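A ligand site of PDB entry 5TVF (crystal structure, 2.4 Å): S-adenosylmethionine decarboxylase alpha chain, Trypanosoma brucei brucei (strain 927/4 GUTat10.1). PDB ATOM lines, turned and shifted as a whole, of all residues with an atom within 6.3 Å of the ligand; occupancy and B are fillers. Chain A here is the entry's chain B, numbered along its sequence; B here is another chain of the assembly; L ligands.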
ATOM      1  C   PYR A   1      18.912 -28.189 -31.982  1.00  0.00           C
ATOM      2  O   PYR A   1      19.411 -28.957 -31.235  1.00  0.00           O
ATOM      3  CA  PYR A   1      18.633 -26.747 -31.567  1.00  0.00           C
ATOM      4  O3  PYR A   1      19.460 -25.913 -31.723  1.00  0.00           O
ATOM      5  CB  PYR A   1      17.294 -26.385 -30.944  1.00  0.00           C
ATOM      6  N   SER A   2      18.494 -28.528 -33.204  1.00  0.00           N
ATOM      7  CA  SER A   2      18.658 -29.877 -33.742  1.00  0.00           C
ATOM      8  C   SER A   2      18.902 -29.833 -35.239  1.00  0.00           C
ATOM      9  O   SER A   2      18.373 -28.974 -35.947  1.00  0.00           O
ATOM     10  CB  SER A   2      17.432 -30.735 -33.438  1.00  0.00           C
ATOM     11  OG  SER A   2      17.283 -30.966 -32.049  1.00  0.00           O
ATOM     12  N   THR A  14      16.253 -24.502 -34.697  1.00  0.00           N
ATOM     13  CA  THR A  14      17.051 -23.615 -33.870  1.00  0.00           C
ATOM     14  C   THR A  14      16.126 -22.785 -32.990  1.00  0.00           C
ATOM     15  O   THR A  14      14.951 -22.566 -33.318  1.00  0.00           O
ATOM     16  CB  THR A  14      17.953 -22.701 -34.705  1.00  0.00           C
ATOM     17  OG1 THR A  14      17.130 -21.822 -35.495  1.00  0.00           O
ATOM     18  CG2 THR A  14      18.831 -23.520 -35.634  1.00  0.00           C
ATOM     19  N   CYS A  15      16.672 -22.316 -31.874  1.00  0.00           N
ATOM     20  CA  CYS A  15      15.922 -21.463 -30.954  1.00  0.00           C
ATOM     21  C   CYS A  15      16.739 -20.222 -30.606  1.00  0.00           C
ATOM     22  O   CYS A  15      17.746 -19.937 -31.257  1.00  0.00           O
ATOM     23  CB  CYS A  15      15.548 -22.244 -29.693  1.00  0.00           C
ATOM     24  SG  CYS A  15      16.936 -23.048 -28.880  1.00  0.00           S
ATOM     25  N   LEU A 156      21.141 -33.326 -23.498  1.00  0.00           N
ATOM     26  CA  LEU A 156      22.095 -32.388 -22.916  1.00  0.00           C
ATOM     27  C   LEU A 156      21.364 -31.525 -21.893  1.00  0.00           C
ATOM     28  O   LEU A 156      20.393 -30.839 -22.237  1.00  0.00           O
ATOM     29  CB  LEU A 156      22.736 -31.514 -23.992  1.00  0.00           C
ATOM     30  CG  LEU A 156      23.660 -30.401 -23.497  1.00  0.00           C
ATOM     31  CD1 LEU A 156      24.847 -30.974 -22.723  1.00  0.00           C
ATOM     32  CD2 LEU A 156      24.144 -29.545 -24.664  1.00  0.00           C
ATOM     33  N   TYR A 158      21.538 -28.275 -19.709  1.00  0.00           N
ATOM     34  CA  TYR A 158      22.257 -27.016 -19.811  1.00  0.00           C
ATOM     35  C   TYR A 158      22.474 -26.392 -18.439  1.00  0.00           C
ATOM     36  O   TYR A 158      21.832 -26.755 -17.439  1.00  0.00           O
ATOM     37  CB  TYR A 158      21.500 -26.038 -20.710  1.00  0.00           C
ATOM     38  CG  TYR A 158      21.582 -26.378 -22.182  1.00  0.00           C
ATOM     39  CD1 TYR A 158      20.777 -27.355 -22.730  1.00  0.00           C
ATOM     40  CD2 TYR A 158      22.464 -25.700 -23.018  1.00  0.00           C
ATOM     41  CE1 TYR A 158      20.852 -27.659 -24.080  1.00  0.00           C
ATOM     42  CE2 TYR A 158      22.541 -25.997 -24.361  1.00  0.00           C
ATOM     43  CZ  TYR A 158      21.741 -26.982 -24.887  1.00  0.00           C
ATOM     44  OH  TYR A 158      21.809 -27.282 -26.225  1.00  0.00           O
ATOM     45  N   GLU A 159      23.392 -25.434 -18.388  1.00  0.00           N
ATOM     46  CA  GLU A 159      23.675 -24.680 -17.186  1.00  0.00           C
ATOM     47  C   GLU A 159      23.385 -23.198 -17.456  1.00  0.00           C
ATOM     48  O   GLU A 159      23.842 -22.660 -18.467  1.00  0.00           O
ATOM     49  CB  GLU A 159      25.129 -24.875 -16.746  1.00  0.00           C
ATOM     50  CG  GLU A 159      25.458 -24.339 -15.355  1.00  0.00           C
ATOM     51  CD  GLU A 159      25.696 -22.844 -15.334  1.00  0.00           C
ATOM     52  OE1 GLU A 159      25.990 -22.262 -16.397  1.00  0.00           O
ATOM     53  OE2 GLU A 159      25.611 -22.247 -14.239  1.00  0.00           O
ATOM     54  N   PRO A 160      22.640 -22.529 -16.563  1.00  0.00           N
ATOM     55  CA  PRO A 160      22.042 -23.027 -15.317  1.00  0.00           C
ATOM     56  C   PRO A 160      20.769 -23.840 -15.541  1.00  0.00           C
ATOM     57  O   PRO A 160      20.384 -24.617 -14.654  1.00  0.00           O
ATOM     58  CB  PRO A 160      21.728 -21.733 -14.545  1.00  0.00           C
ATOM     59  CG  PRO A 160      21.462 -20.739 -15.612  1.00  0.00           C
ATOM     60  CD  PRO A 160      22.366 -21.096 -16.757  1.00  0.00           C
ATOM     61  N   CYS A 161      20.119 -23.674 -16.687  1.00  0.00           N
ATOM     62  CA  CYS A 161      18.900 -24.404 -16.989  1.00  0.00           C
ATOM     63  C   CYS A 161      18.789 -24.584 -18.498  1.00  0.00           C
ATOM     64  O   CYS A 161      19.473 -23.919 -19.281  1.00  0.00           O
ATOM     65  CB  CYS A 161      17.657 -23.676 -16.451  1.00  0.00           C
ATOM     66  SG  CYS A 161      17.471 -21.973 -17.032  1.00  0.00           S
ATOM     67  N   GLY A 162      17.908 -25.501 -18.897  1.00  0.00           N
ATOM     68  CA  GLY A 162      17.713 -25.841 -20.289  1.00  0.00           C
ATOM     69  C   GLY A 162      17.988 -27.309 -20.562  1.00  0.00           C
ATOM     70  O   GLY A 162      18.943 -27.872 -20.026  1.00  0.00           O
ATOM     71  N   TYR A 163      17.165 -27.931 -21.399  1.00  0.00           N
ATOM     72  CA  TYR A 163      17.300 -29.350 -21.704  1.00  0.00           C
ATOM     73  C   TYR A 163      16.943 -29.607 -23.160  1.00  0.00           C
ATOM     74  O   TYR A 163      15.954 -29.068 -23.668  1.00  0.00           O
ATOM     75  CB  TYR A 163      16.404 -30.202 -20.789  1.00  0.00           C
ATOM     76  CG  TYR A 163      16.441 -31.688 -21.099  1.00  0.00           C
ATOM     77  CD1 TYR A 163      15.570 -32.241 -22.029  1.00  0.00           C
ATOM     78  CD2 TYR A 163      17.343 -32.527 -20.461  1.00  0.00           C
ATOM     79  CE1 TYR A 163      15.586 -33.586 -22.308  1.00  0.00           C
ATOM     80  CE2 TYR A 163      17.365 -33.885 -20.742  1.00  0.00           C
ATOM     81  CZ  TYR A 163      16.492 -34.401 -21.666  1.00  0.00           C
ATOM     82  OH  TYR A 163      16.514 -35.759 -21.947  1.00  0.00           O
ATOM     83  N   SER A 164      17.761 -30.412 -23.822  1.00  0.00           N
ATOM     84  CA  SER A 164      17.512 -30.852 -25.193  1.00  0.00           C
ATOM     85  C   SER A 164      17.693 -32.356 -25.273  1.00  0.00           C
ATOM     86  O   SER A 164      18.475 -32.942 -24.519  1.00  0.00           O
ATOM     87  CB  SER A 164      18.455 -30.161 -26.192  1.00  0.00           C
ATOM     88  OG  SER A 164      18.267 -28.762 -26.204  1.00  0.00           O
ATOM     89  N   ILE A 176      12.943 -32.923 -28.423  1.00  0.00           N
ATOM     90  CA  ILE A 176      12.311 -32.107 -27.395  1.00  0.00           C
ATOM     91  C   ILE A 176      13.317 -31.068 -26.922  1.00  0.00           C
ATOM     92  O   ILE A 176      14.503 -31.352 -26.773  1.00  0.00           O
ATOM     93  CB  ILE A 176      11.812 -32.963 -26.212  1.00  0.00           C
ATOM     94  CG1 ILE A 176      10.589 -33.786 -26.633  1.00  0.00           C
ATOM     95  CG2 ILE A 176      11.476 -32.088 -24.995  1.00  0.00           C
ATOM     96  CD1 ILE A 176      10.098 -34.755 -25.566  1.00  0.00           C
ATOM     97  N   HIS A 177      12.828 -29.845 -26.672  1.00  0.00           N
ATOM     98  CA  HIS A 177      13.651 -28.768 -26.143  1.00  0.00           C
ATOM     99  C   HIS A 177      12.844 -28.002 -25.111  1.00  0.00           C
ATOM    100  O   HIS A 177      11.689 -27.648 -25.365  1.00  0.00           O
ATOM    101  CB  HIS A 177      14.111 -27.834 -27.270  1.00  0.00           C
ATOM    102  CG  HIS A 177      14.851 -28.540 -28.368  1.00  0.00           C
ATOM    103  ND1 HIS A 177      16.224 -28.659 -28.368  1.00  0.00           N
ATOM    104  CD2 HIS A 177      14.414 -29.165 -29.481  1.00  0.00           C
ATOM    105  CE1 HIS A 177      16.604 -29.330 -29.440  1.00  0.00           C
ATOM    106  NE2 HIS A 177      15.526 -29.647 -30.139  1.00  0.00           N
ATOM    107  N   ILE A 178      13.443 -27.756 -23.949  1.00  0.00           N
ATOM    108  CA  ILE A 178      12.735 -27.258 -22.786  1.00  0.00           C
ATOM    109  C   ILE A 178      13.390 -25.964 -22.313  1.00  0.00           C
ATOM    110  O   ILE A 178      14.627 -25.889 -22.206  1.00  0.00           O
ATOM    111  CB  ILE A 178      12.710 -28.294 -21.653  1.00  0.00           C
ATOM    112  CG1 ILE A 178      12.069 -29.596 -22.150  1.00  0.00           C
ATOM    113  CG2 ILE A 178      11.957 -27.750 -20.446  1.00  0.00           C
ATOM    114  CD1 ILE A 178      12.119 -30.738 -21.162  1.00  0.00           C
ATOM    115  N   THR A 179      12.567 -24.957 -22.013  1.00  0.00           N
ATOM    116  CA  THR A 179      13.014 -23.733 -21.355  1.00  0.00           C
ATOM    117  C   THR A 179      12.226 -23.618 -20.050  1.00  0.00           C
ATOM    118  O   THR A 179      11.031 -23.261 -20.072  1.00  0.00           O
ATOM    119  CB  THR A 179      12.773 -22.508 -22.245  1.00  0.00           C
ATOM    120  OG1 THR A 179      13.562 -22.630 -23.429  1.00  0.00           O
ATOM    121  CG2 THR A 179      13.155 -21.227 -21.507  1.00  0.00           C
ATOM    122  N   PRO A 180      12.834 -23.900 -18.894  1.00  0.00           N
ATOM    123  CA  PRO A 180      12.037 -24.060 -17.665  1.00  0.00           C
ATOM    124  C   PRO A 180      11.828 -22.802 -16.828  1.00  0.00           C
ATOM    125  O   PRO A 180      11.077 -22.885 -15.841  1.00  0.00           O
ATOM    126  CB  PRO A 180      12.869 -25.089 -16.867  1.00  0.00           C
ATOM    127  CG  PRO A 180      14.206 -25.197 -17.576  1.00  0.00           C
ATOM    128  CD  PRO A 180      14.259 -24.138 -18.621  1.00  0.00           C
ATOM    129  N   GLU A 181      12.442 -21.677 -17.167  1.00  0.00           N
ATOM    130  CA  GLU A 181      12.231 -20.449 -16.398  1.00  0.00           C
ATOM    131  C   GLU A 181      10.735 -20.228 -16.170  1.00  0.00           C
ATOM    132  O   GLU A 181       9.921 -20.366 -17.086  1.00  0.00           O
ATOM    133  CB  GLU A 181      12.826 -19.245 -17.131  1.00  0.00           C
ATOM    134  CG  GLU A 181      14.343 -19.197 -17.119  1.00  0.00           C
ATOM    135  CD  GLU A 181      14.974 -19.970 -18.263  1.00  0.00           C
ATOM    136  OE1 GLU A 181      14.376 -20.965 -18.706  1.00  0.00           O
ATOM    137  OE2 GLU A 181      16.057 -19.566 -18.716  1.00  0.00           O
ATOM    138  N   PHE B  28      14.436 -16.108 -22.208  1.00  0.00           N
ATOM    139  CA  PHE B  28      14.983 -16.829 -23.352  1.00  0.00           C
ATOM    140  C   PHE B  28      13.878 -17.173 -24.349  1.00  0.00           C
ATOM    141  O   PHE B  28      12.727 -17.411 -23.970  1.00  0.00           O
ATOM    142  CB  PHE B  28      15.689 -18.100 -22.891  1.00  0.00           C
ATOM    143  CG  PHE B  28      16.267 -18.918 -24.012  1.00  0.00           C
ATOM    144  CD1 PHE B  28      17.520 -18.627 -24.515  1.00  0.00           C
ATOM    145  CD2 PHE B  28      15.552 -19.960 -24.563  1.00  0.00           C
ATOM    146  CE1 PHE B  28      18.051 -19.367 -25.551  1.00  0.00           C
ATOM    147  CE2 PHE B  28      16.074 -20.710 -25.601  1.00  0.00           C
ATOM    148  CZ  PHE B  28      17.328 -20.412 -26.098  1.00  0.00           C
ATOM    149  N   GLU B  32      10.863 -21.988 -31.640  1.00  0.00           N
ATOM    150  CA  GLU B  32      11.970 -22.340 -32.501  1.00  0.00           C
ATOM    151  C   GLU B  32      11.698 -21.942 -33.948  1.00  0.00           C
ATOM    152  O   GLU B  32      10.553 -21.739 -34.364  1.00  0.00           O
ATOM    153  CB  GLU B  32      12.239 -23.842 -32.451  1.00  0.00           C
ATOM    154  CG  GLU B  32      12.535 -24.361 -31.056  1.00  0.00           C
ATOM    155  CD  GLU B  32      12.138 -25.812 -30.872  1.00  0.00           C
ATOM    156  OE1 GLU B  32      11.544 -26.381 -31.806  1.00  0.00           O
ATOM    157  OE2 GLU B  32      12.415 -26.363 -29.786  1.00  0.00           O
ATOM    158  N   VAL B  82      22.893 -32.626 -32.033  1.00  0.00           N
ATOM    159  CA  VAL B  82      22.438 -31.662 -31.034  1.00  0.00           C
ATOM    160  C   VAL B  82      23.287 -30.411 -31.173  1.00  0.00           C
ATOM    161  O   VAL B  82      24.511 -30.489 -31.353  1.00  0.00           O
ATOM    162  CB  VAL B  82      22.530 -32.233 -29.602  1.00  0.00           C
ATOM    163  CG1 VAL B  82      22.103 -31.187 -28.577  1.00  0.00           C
ATOM    164  CG2 VAL B  82      21.683 -33.482 -29.479  1.00  0.00           C
ATOM    165  N   LEU B  83      22.646 -29.252 -31.125  1.00  0.00           N
ATOM    166  CA  LEU B  83      23.302 -27.974 -31.339  1.00  0.00           C
ATOM    167  C   LEU B  83      23.153 -27.089 -30.113  1.00  0.00           C
ATOM    168  O   LEU B  83      22.249 -27.279 -29.300  1.00  0.00           O
ATOM    169  CB  LEU B  83      22.728 -27.266 -32.575  1.00  0.00           C
ATOM    170  CG  LEU B  83      22.560 -28.155 -33.813  1.00  0.00           C
ATOM    171  CD1 LEU B  83      21.862 -27.388 -34.920  1.00  0.00           C
ATOM    172  CD2 LEU B  83      23.907 -28.683 -34.296  1.00  0.00           C
ATOM    173  N   SER B  84      24.043 -26.113 -29.992  1.00  0.00           N
ATOM    174  CA  SER B  84      23.998 -25.165 -28.901  1.00  0.00           C
ATOM    175  C   SER B  84      24.607 -23.853 -29.359  1.00  0.00           C
ATOM    176  O   SER B  84      25.585 -23.847 -30.124  1.00  0.00           O
ATOM    177  CB  SER B  84      24.734 -25.682 -27.666  1.00  0.00           C
ATOM    178  OG  SER B  84      24.567 -24.812 -26.567  1.00  0.00           O
ATOM    179  N   GLU B  85      24.045 -22.744 -28.897  1.00  0.00           N
ATOM    180  CA  GLU B  85      24.515 -21.418 -29.264  1.00  0.00           C
ATOM    181  C   GLU B  85      26.001 -21.253 -28.938  1.00  0.00           C
ATOM    182  O   GLU B  85      26.577 -22.032 -28.175  1.00  0.00           O
ATOM    183  CB  GLU B  85      23.707 -20.335 -28.542  1.00  0.00           C
ATOM    184  CG  GLU B  85      22.225 -20.319 -28.911  1.00  0.00           C
ATOM    185  CD  GLU B  85      21.489 -19.141 -28.311  1.00  0.00           C
ATOM    186  OE1 GLU B  85      21.928 -18.646 -27.252  1.00  0.00           O
ATOM    187  OE2 GLU B  85      20.470 -18.711 -28.889  1.00  0.00           O
ATOM    188  OXT GLU B  85      26.665 -20.340 -29.440  1.00  0.00           O
HETATM  189  C1  LIG L   1      23.230 -17.834 -20.027  1.00  0.00           C
HETATM  190  C2  LIG L   1      22.183 -18.736 -20.190  1.00  0.00           C
HETATM  191  C3  LIG L   1      21.135 -18.732 -19.283  1.00  0.00           C
HETATM  192  C4  LIG L   1      21.121 -17.828 -18.237  1.00  0.00           C
HETATM  193  C5  LIG L   1      22.167 -16.933 -18.082  1.00  0.00           C
HETATM  194  C6  LIG L   1      23.222 -16.936 -18.977  1.00  0.00           C
HETATM  195  C7  LIG L   1      19.966 -19.707 -19.412  1.00  0.00           C
HETATM  196  N1  LIG L   1      18.980 -19.372 -20.113  1.00  0.00           N
HETATM  197  C8  LIG L   1      24.410 -17.803 -21.002  1.00  0.00           C
HETATM  198  N2  LIG L   1      25.137 -19.006 -21.361  1.00  0.00           N
HETATM  199  N3  LIG L   1      24.760 -16.706 -21.493  1.00  0.00           N
HETATM  200  N4  LIG L   1      17.858 -20.232 -20.222  1.00  0.00           N
HETATM  201  C9  LIG L   1      17.837 -21.409 -21.071  1.00  0.00           C
HETATM  202  N5  LIG L   1      16.609 -22.193 -21.071  1.00  0.00           N
HETATM  203  N6  LIG L   1      18.807 -21.765 -21.767  1.00  0.00           N
HETATM  204  N7  LIG L   1      18.642 -22.927 -22.553  1.00  0.00           N
HETATM  205  C10 LIG L   1      18.111 -22.773 -23.675  1.00  0.00           C
HETATM  206  C11 LIG L   1      17.838 -23.941 -24.628  1.00  0.00           C
HETATM  207  C12 LIG L   1      16.659 -24.643 -24.460  1.00  0.00           C
HETATM  208  C13 LIG L   1      16.343 -25.697 -25.294  1.00  0.00           C
HETATM  209  C14 LIG L   1      17.215 -26.043 -26.318  1.00  0.00           C
HETATM  210  C15 LIG L   1      18.395 -25.338 -26.502  1.00  0.00           C
HETATM  211  C16 LIG L   1      18.712 -24.277 -25.661  1.00  0.00           C
HETATM  212  C17 LIG L   1      19.308 -25.768 -27.646  1.00  0.00           C
HETATM  213  N8  LIG L   1      19.871 -24.804 -28.575  1.00  0.00           N
HETATM  214  N9  LIG L   1      19.556 -26.988 -27.797  1.00  0.00           N
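N5 of the ligand is in salt-bridge range of OE1 of Glu 181. A nitrogen (N9) of the ligand sits at hydrogen-bond distance from the side-chain hydroxyl (OG) of Ser 164. N9 of the ligand sits at hydrogen-bond distance from OH of Tyr 158 (2.8 Å). O of Leu 83 of chain B is in hydrogen-bond range of N9 of the ligand (3.1 Å). The backbone carbonyl oxygen of Cys 161 lies within hydrogen-bond range of a nitrogen (N6) of the ligand (3.4 Å). SG of Cys 161 lies within hydrogen-bond range of N4 of the ligand. O3 of PYR 1 sits at hydrogen-bond distance from N8 of the ligand, 3.4 Å away. The side-chain sulfur (SG) of Cys 15 lies within hydrogen-bond range of a nitrogen (N8) of the ligand.
The side-chain sulfur (SG) of Cys 161 lies within hydrogen-bond range of the side-chain carboxylate (OE2) of Glu 181. OG of Ser 164 is in hydrogen-bond range of ND1 of His 177, 3.0 Å away. The backbone NH (N) of Leu 156 is in hydrogen-bond range of the backbone carbonyl oxygen (O) of Ser 164. OH of Tyr 158 sits at hydrogen-bond distance from O of Leu 83 of chain B. N of Leu 83 of chain B is in hydrogen-bond range of O of PYR 1 (3.3 Å). The backbone carbonyl oxygen (O) of Tyr 163 is in hydrogen-bond range of the backbone NH (N) of Ile 178 (2.8 Å). A ring nitrogen (NE2) of His 177 sits at hydrogen-bond distance from the side-chain hydroxyl (OG) of Ser 2 (2.9 Å).
Residues that only touch the ligand: Pro 160, Gly 162, Tyr 163, His 177, Ile 178, Thr 179, Pro 180 and Phe 28 of chain B. Hydrophobic or aromatic side chains within 4 Å of the ligand: Tyr 158, Pro 160, His 177, Pro 180 and Phe 28 of chain B. Of the 24 residues printed, 15 come within 4 Å of the ligand.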
